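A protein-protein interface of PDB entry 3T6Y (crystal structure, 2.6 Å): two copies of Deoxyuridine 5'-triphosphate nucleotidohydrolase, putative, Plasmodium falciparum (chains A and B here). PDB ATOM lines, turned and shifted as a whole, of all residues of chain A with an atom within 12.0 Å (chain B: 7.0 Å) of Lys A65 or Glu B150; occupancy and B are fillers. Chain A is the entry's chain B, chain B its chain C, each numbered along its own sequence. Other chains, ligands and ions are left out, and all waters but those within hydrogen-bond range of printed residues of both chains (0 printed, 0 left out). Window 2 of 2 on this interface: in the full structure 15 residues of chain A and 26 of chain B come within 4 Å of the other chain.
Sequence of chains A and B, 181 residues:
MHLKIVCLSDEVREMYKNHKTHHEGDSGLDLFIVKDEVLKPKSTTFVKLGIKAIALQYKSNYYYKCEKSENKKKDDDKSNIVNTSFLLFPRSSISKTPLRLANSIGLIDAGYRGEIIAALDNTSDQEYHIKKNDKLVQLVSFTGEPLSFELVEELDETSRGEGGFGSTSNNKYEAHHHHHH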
ATOM      1  N   ASN A  61     -22.993  11.319 -17.448  1.00  0.00           N
ATOM      2  CA  ASN A  61     -23.012  11.988 -16.157  1.00  0.00           C
ATOM      3  C   ASN A  61     -21.914  13.054 -16.206  1.00  0.00           C
ATOM      4  O   ASN A  61     -20.741  12.759 -16.503  1.00  0.00           O
ATOM      5  CB  ASN A  61     -22.734  11.019 -14.994  1.00  0.00           C
ATOM      6  CG  ASN A  61     -23.708   9.849 -14.938  1.00  0.00           C
ATOM      7  OD1 ASN A  61     -24.925  10.033 -14.829  1.00  0.00           O
ATOM      8  ND2 ASN A  61     -23.165   8.626 -14.988  1.00  0.00           N
ATOM      9  N   TYR A  62     -22.312  14.291 -15.940  1.00  0.00           N
ATOM     10  CA  TYR A  62     -21.388  15.410 -15.768  1.00  0.00           C
ATOM     11  C   TYR A  62     -21.683  16.083 -14.423  1.00  0.00           C
ATOM     12  O   TYR A  62     -22.830  16.198 -14.046  1.00  0.00           O
ATOM     13  CB  TYR A  62     -21.533  16.418 -16.932  1.00  0.00           C
ATOM     14  CG  TYR A  62     -22.931  17.010 -17.198  1.00  0.00           C
ATOM     15  CD1 TYR A  62     -23.399  18.153 -16.501  1.00  0.00           C
ATOM     16  CD2 TYR A  62     -23.767  16.467 -18.201  1.00  0.00           C
ATOM     17  CE1 TYR A  62     -24.667  18.693 -16.777  1.00  0.00           C
ATOM     18  CE2 TYR A  62     -25.031  17.004 -18.491  1.00  0.00           C
ATOM     19  CZ  TYR A  62     -25.490  18.101 -17.778  1.00  0.00           C
ATOM     20  OH  TYR A  62     -26.750  18.619 -18.078  1.00  0.00           O
ATOM     21  N   TYR A  63     -20.671  16.549 -13.709  1.00  0.00           N
ATOM     22  CA  TYR A  63     -20.933  17.228 -12.453  1.00  0.00           C
ATOM     23  C   TYR A  63     -21.456  18.630 -12.709  1.00  0.00           C
ATOM     24  O   TYR A  63     -20.864  19.363 -13.476  1.00  0.00           O
ATOM     25  CB  TYR A  63     -19.682  17.256 -11.584  1.00  0.00           C
ATOM     26  CG  TYR A  63     -19.909  17.868 -10.207  1.00  0.00           C
ATOM     27  CD1 TYR A  63     -20.836  17.319  -9.301  1.00  0.00           C
ATOM     28  CD2 TYR A  63     -19.207  19.008  -9.813  1.00  0.00           C
ATOM     29  CE1 TYR A  63     -21.034  17.894  -8.052  1.00  0.00           C
ATOM     30  CE2 TYR A  63     -19.401  19.587  -8.574  1.00  0.00           C
ATOM     31  CZ  TYR A  63     -20.303  19.027  -7.692  1.00  0.00           C
ATOM     32  OH  TYR A  63     -20.478  19.632  -6.463  1.00  0.00           O
ATOM     33  N   TYR A  64     -22.566  19.010 -12.069  1.00  0.00           N
ATOM     34  CA  TYR A  64     -23.172  20.351 -12.266  1.00  0.00           C
ATOM     35  C   TYR A  64     -24.087  20.731 -11.098  1.00  0.00           C
ATOM     36  O   TYR A  64     -24.797  19.871 -10.591  1.00  0.00           O
ATOM     37  CB  TYR A  64     -23.955  20.359 -13.585  1.00  0.00           C
ATOM     38  CG  TYR A  64     -24.647  21.651 -14.028  1.00  0.00           C
ATOM     39  CD1 TYR A  64     -25.841  22.089 -13.417  1.00  0.00           C
ATOM     40  CD2 TYR A  64     -24.162  22.390 -15.128  1.00  0.00           C
ATOM     41  CE1 TYR A  64     -26.496  23.244 -13.856  1.00  0.00           C
ATOM     42  CE2 TYR A  64     -24.812  23.535 -15.582  1.00  0.00           C
ATOM     43  CZ  TYR A  64     -25.976  23.956 -14.948  1.00  0.00           C
ATOM     44  OH  TYR A  64     -26.621  25.082 -15.378  1.00  0.00           O
ATOM     45  N   LYS A  65     -24.074  22.003 -10.677  1.00  0.00           N
ATOM     46  CA  LYS A  65     -24.949  22.493  -9.584  1.00  0.00           C
ATOM     47  C   LYS A  65     -25.821  23.694  -9.960  1.00  0.00           C
ATOM     48  O   LYS A  65     -27.046  23.562 -10.073  1.00  0.00           O
ATOM     49  CB  LYS A  65     -24.127  22.841  -8.352  1.00  0.00           C
ATOM     50  CG  LYS A  65     -23.172  21.741  -7.895  1.00  0.00           C
ATOM     51  CD  LYS A  65     -22.840  21.922  -6.428  1.00  0.00           C
ATOM     52  CE  LYS A  65     -23.249  23.336  -6.010  1.00  0.00           C
ATOM     53  NZ  LYS A  65     -22.391  23.943  -4.961  1.00  0.00           N
ATOM     54  N   MET B   1     -19.696  20.526 -15.605  1.00  0.00           N
ATOM     55  CA  MET B   1     -18.488  20.937 -14.872  1.00  0.00           C
ATOM     56  C   MET B   1     -18.938  22.036 -13.980  1.00  0.00           C
ATOM     57  O   MET B   1     -19.825  22.792 -14.344  1.00  0.00           O
ATOM     58  CB  MET B   1     -17.469  21.464 -15.833  1.00  0.00           C
ATOM     59  CG  MET B   1     -16.140  21.805 -15.199  1.00  0.00           C
ATOM     60  SD  MET B   1     -14.906  22.260 -16.451  1.00  0.00           S
ATOM     61  CE  MET B   1     -15.177  24.044 -16.522  1.00  0.00           C
ATOM     62  N   HIS B   2     -18.336  22.124 -12.806  1.00  0.00           N
ATOM     63  CA  HIS B   2     -18.696  23.147 -11.867  1.00  0.00           C
ATOM     64  C   HIS B   2     -17.481  23.890 -11.483  1.00  0.00           C
ATOM     65  O   HIS B   2     -16.466  23.271 -11.173  1.00  0.00           O
ATOM     66  CB  HIS B   2     -19.323  22.482 -10.651  1.00  0.00           C
ATOM     67  CG  HIS B   2     -19.734  23.442  -9.578  1.00  0.00           C
ATOM     68  ND1 HIS B   2     -20.764  24.312  -9.741  1.00  0.00           N
ATOM     69  CD2 HIS B   2     -19.193  23.678  -8.319  1.00  0.00           C
ATOM     70  CE1 HIS B   2     -20.893  25.048  -8.617  1.00  0.00           C
ATOM     71  NE2 HIS B   2     -19.933  24.643  -7.741  1.00  0.00           N
ATOM     72  N   LEU B   3     -17.544  25.214 -11.485  1.00  0.00           N
ATOM     73  CA  LEU B   3     -16.383  26.071 -11.175  1.00  0.00           C
ATOM     74  C   LEU B   3     -16.581  26.745  -9.838  1.00  0.00           C
ATOM     75  O   LEU B   3     -17.665  27.230  -9.578  1.00  0.00           O
ATOM     76  CB  LEU B   3     -16.234  27.187 -12.221  1.00  0.00           C
ATOM     77  CG  LEU B   3     -15.728  26.879 -13.617  1.00  0.00           C
ATOM     78  CD1 LEU B   3     -16.459  27.739 -14.608  1.00  0.00           C
ATOM     79  CD2 LEU B   3     -14.253  27.171 -13.745  1.00  0.00           C
ATOM     80  N   LYS B   4     -15.535  26.790  -9.021  1.00  0.00           N
ATOM     81  CA  LYS B   4     -15.472  27.639  -7.838  1.00  0.00           C
ATOM     82  C   LYS B   4     -14.598  28.850  -8.148  1.00  0.00           C
ATOM     83  O   LYS B   4     -13.436  28.694  -8.447  1.00  0.00           O
ATOM     84  CB  LYS B   4     -14.834  26.872  -6.707  1.00  0.00           C
ATOM     85  CG  LYS B   4     -15.512  25.554  -6.521  1.00  0.00           C
ATOM     86  CD  LYS B   4     -15.273  24.900  -5.191  1.00  0.00           C
ATOM     87  CE  LYS B   4     -16.602  24.245  -4.814  1.00  0.00           C
ATOM     88  NZ  LYS B   4     -16.547  23.357  -3.616  1.00  0.00           N
ATOM     89  N   ILE B   5     -15.174  30.047  -8.075  1.00  0.00           N
ATOM     90  CA  ILE B   5     -14.528  31.278  -8.486  1.00  0.00           C
ATOM     91  C   ILE B   5     -14.313  32.183  -7.278  1.00  0.00           C
ATOM     92  O   ILE B   5     -15.265  32.556  -6.607  1.00  0.00           O
ATOM     93  CB  ILE B   5     -15.442  32.016  -9.451  1.00  0.00           C
ATOM     94  CG1 ILE B   5     -15.541  31.232 -10.739  1.00  0.00           C
ATOM     95  CG2 ILE B   5     -14.922  33.396  -9.756  1.00  0.00           C
ATOM     96  CD1 ILE B   5     -16.700  31.710 -11.591  1.00  0.00           C
ATOM     97  N   VAL B   6     -13.070  32.512  -6.976  1.00  0.00           N
ATOM     98  CA  VAL B   6     -12.791  33.502  -5.975  1.00  0.00           C
ATOM     99  C   VAL B   6     -12.655  34.854  -6.649  1.00  0.00           C
ATOM    100  O   VAL B   6     -11.747  35.031  -7.452  1.00  0.00           O
ATOM    101  CB  VAL B   6     -11.445  33.228  -5.316  1.00  0.00           C
ATOM    102  CG1 VAL B   6     -11.236  34.192  -4.186  1.00  0.00           C
ATOM    103  CG2 VAL B   6     -11.396  31.828  -4.774  1.00  0.00           C
ATOM    104  N   LEU B  56     -14.411  21.390 -11.346  1.00  0.00           N
ATOM    105  CA  LEU B  56     -14.648  20.077 -10.746  1.00  0.00           C
ATOM    106  C   LEU B  56     -15.459  19.252 -11.702  1.00  0.00           C
ATOM    107  O   LEU B  56     -16.411  19.780 -12.297  1.00  0.00           O
ATOM    108  CB  LEU B  56     -15.414  20.188  -9.430  1.00  0.00           C
ATOM    109  CG  LEU B  56     -14.817  20.644  -8.084  1.00  0.00           C
ATOM    110  CD1 LEU B  56     -13.322  20.432  -7.922  1.00  0.00           C
ATOM    111  CD2 LEU B  56     -15.122  22.094  -7.858  1.00  0.00           C
ATOM    112  N   LEU B 147     -21.823  24.303 -17.759  1.00  0.00           N
ATOM    113  CA  LEU B 147     -21.035  24.807 -16.641  1.00  0.00           C
ATOM    114  C   LEU B 147     -21.900  25.447 -15.588  1.00  0.00           C
ATOM    115  O   LEU B 147     -22.822  26.181 -15.874  1.00  0.00           O
ATOM    116  CB  LEU B 147     -20.007  25.873 -17.061  1.00  0.00           C
ATOM    117  CG  LEU B 147     -18.873  25.568 -18.053  1.00  0.00           C
ATOM    118  CD1 LEU B 147     -17.685  26.513 -17.846  1.00  0.00           C
ATOM    119  CD2 LEU B 147     -18.400  24.117 -18.038  1.00  0.00           C
ATOM    120  N   SER B 148     -21.564  25.198 -14.340  1.00  0.00           N
ATOM    121  CA  SER B 148     -22.250  25.830 -13.251  1.00  0.00           C
ATOM    122  C   SER B 148     -21.137  26.505 -12.443  1.00  0.00           C
ATOM    123  O   SER B 148     -19.998  26.062 -12.494  1.00  0.00           O
ATOM    124  CB  SER B 148     -23.053  24.765 -12.458  1.00  0.00           C
ATOM    125  OG  SER B 148     -22.241  23.847 -11.712  1.00  0.00           O
ATOM    126  N   PHE B 149     -21.410  27.577 -11.725  1.00  0.00           N
ATOM    127  CA  PHE B 149     -20.359  28.067 -10.854  1.00  0.00           C
ATOM    128  C   PHE B 149     -20.882  28.557  -9.502  1.00  0.00           C
ATOM    129  O   PHE B 149     -22.058  28.712  -9.329  1.00  0.00           O
ATOM    130  CB  PHE B 149     -19.611  29.182 -11.559  1.00  0.00           C
ATOM    131  CG  PHE B 149     -20.427  30.427 -11.760  1.00  0.00           C
ATOM    132  CD1 PHE B 149     -21.333  30.514 -12.797  1.00  0.00           C
ATOM    133  CD2 PHE B 149     -20.264  31.534 -10.902  1.00  0.00           C
ATOM    134  CE1 PHE B 149     -22.091  31.658 -12.967  1.00  0.00           C
ATOM    135  CE2 PHE B 149     -21.012  32.687 -11.073  1.00  0.00           C
ATOM    136  CZ  PHE B 149     -21.938  32.748 -12.110  1.00  0.00           C
ATOM    137  N   GLU B 150     -19.996  28.812  -8.549  1.00  0.00           N
ATOM    138  CA  GLU B 150     -20.359  29.532  -7.344  1.00  0.00           C
ATOM    139  C   GLU B 150     -19.179  30.366  -6.862  1.00  0.00           C
ATOM    140  O   GLU B 150     -18.011  30.029  -7.107  1.00  0.00           O
ATOM    141  CB  GLU B 150     -20.772  28.572  -6.257  1.00  0.00           C
ATOM    142  CG  GLU B 150     -19.762  27.484  -6.047  1.00  0.00           C
ATOM    143  CD  GLU B 150     -19.976  26.723  -4.762  1.00  0.00           C
ATOM    144  OE1 GLU B 150     -20.373  27.343  -3.746  1.00  0.00           O
ATOM    145  OE2 GLU B 150     -19.715  25.505  -4.770  1.00  0.00           O
ATOM    146  N   LEU B 151     -19.494  31.467  -6.184  1.00  0.00           N
ATOM    147  CA  LEU B 151     -18.476  32.289  -5.600  1.00  0.00           C
ATOM    148  C   LEU B 151     -18.073  31.656  -4.291  1.00  0.00           C
ATOM    149  O   LEU B 151     -18.924  31.236  -3.519  1.00  0.00           O
ATOM    150  CB  LEU B 151     -18.984  33.706  -5.388  1.00  0.00           C
ATOM    151  CG  LEU B 151     -19.730  34.317  -6.574  1.00  0.00           C
ATOM    152  CD1 LEU B 151     -19.888  35.830  -6.369  1.00  0.00           C
ATOM    153  CD2 LEU B 151     -18.921  33.998  -7.825  1.00  0.00           C
ATOM    154  N   VAL B 152     -16.765  31.542  -4.080  1.00  0.00           N
ATOM    155  CA  VAL B 152     -16.225  31.072  -2.829  1.00  0.00           C
ATOM    156  C   VAL B 152     -15.159  32.071  -2.436  1.00  0.00           C
ATOM    157  O   VAL B 152     -14.758  32.871  -3.235  1.00  0.00           O
ATOM    158  CB  VAL B 152     -15.669  29.665  -2.986  1.00  0.00           C
ATOM    159  CG1 VAL B 152     -16.793  28.748  -3.449  1.00  0.00           C
ATOM    160  CG2 VAL B 152     -14.513  29.676  -4.000  1.00  0.00           C
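N of Ile B5 lies within hydrogen-bond range of O of Glu B150 (3.0 Å).
N of Ser B148 is in hydrogen-bond range of O of Met B1, 3.0 Å away.
ND1 of His B2 is in hydrogen-bond range of OG of Ser B148 (2.5 Å).
The backbone NH (N) of Leu B3 lies within hydrogen-bond range of the backbone carbonyl oxygen (O) of Ser B148 (2.8 Å).
NZ of Lys B4 is in salt-bridge range of OE2 of Glu B150.
O of Leu B3 lies within hydrogen-bond range of N of Glu B150, 3.0 Å away.
Of the 5 printed residues of chain A, 3 touch a printed residue of chain B.
Printed residues of chain A that touch a printed residue of chain B: Tyr A63, Tyr A64 and Lys A65.
Along chain A the printed residues that touch a printed residue of chain B span positions 63 to 65.
Printed residues of chain B that touch a printed residue of chain A: Met B1, His B2, Leu B56, Leu B147, Ser B148 and Glu B150.
Hydrophobic or aromatic side chains of chain B that line the printed part of chain A: His B2 and Leu B56.
Among the printed residues, 8 pairs touch across the chains.
Asn A61 touches none of the printed residues of chain B.
Tyr A62 touches none of the printed residues of chain B.
Of the printed residues of chain B, Tyr A63 touches Met B1, His B2 and Leu B56.
Of the printed residues of chain B, Tyr A64 touches Leu B147 (3.3 Å) and Ser B148 (3.7 Å).
Of chain B, only His B2 (3.8 Å), Ser B148 (2.8 Å) and Glu B150 (3.1 Å) come within 4 Å of Lys A65.
Printed residues of chain A within 4 Å of Met B1: Tyr A63.
No residue of chain A comes within 4 Å of Leu B3.
Ile B5 touches none of the printed residues of chain A.
Of the printed residues of chain A, Leu B56 touches Tyr A63 (3.8 Å).
Printed residues of chain A within 4 Å of Leu B147: Tyr A64 (3.3 Å).
Ser B148 touches just these residues of chain A: Tyr A64 (3.7 Å) and Lys A65 (2.8 Å).
No residue of chain A comes within 4 Å of Val B152.
The nearest printed residue of chain A that does not touch Leu B147 is Tyr A63 (6.3 Å).
The side-chain carboxylate (OE2) of Glu B150 is in salt-bridge range of the side-chain amino group (NZ) of Lys A65, 3.1 Å away.
The backbone carbonyl oxygen of Tyr A63 is in hydrogen-bond range of the backbone NH of Met B1 (2.7 Å).
The side-chain hydroxyl (OG) of Ser B148 sits at hydrogen-bond distance from the backbone NH (N) of Lys A65 (2.8 Å).
No position is printed for both chains.
Of the 8 pairs that touch across the chains among the printed residues, none has its exchanged pair printed and touching as well.
Among the printed residues, merely in contact across the chains: Tyr A63 with His B2, Tyr A63 with Leu B56, Tyr A64 with Leu B147, Tyr A64 with Ser B148 and Lys A65 with His B2.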
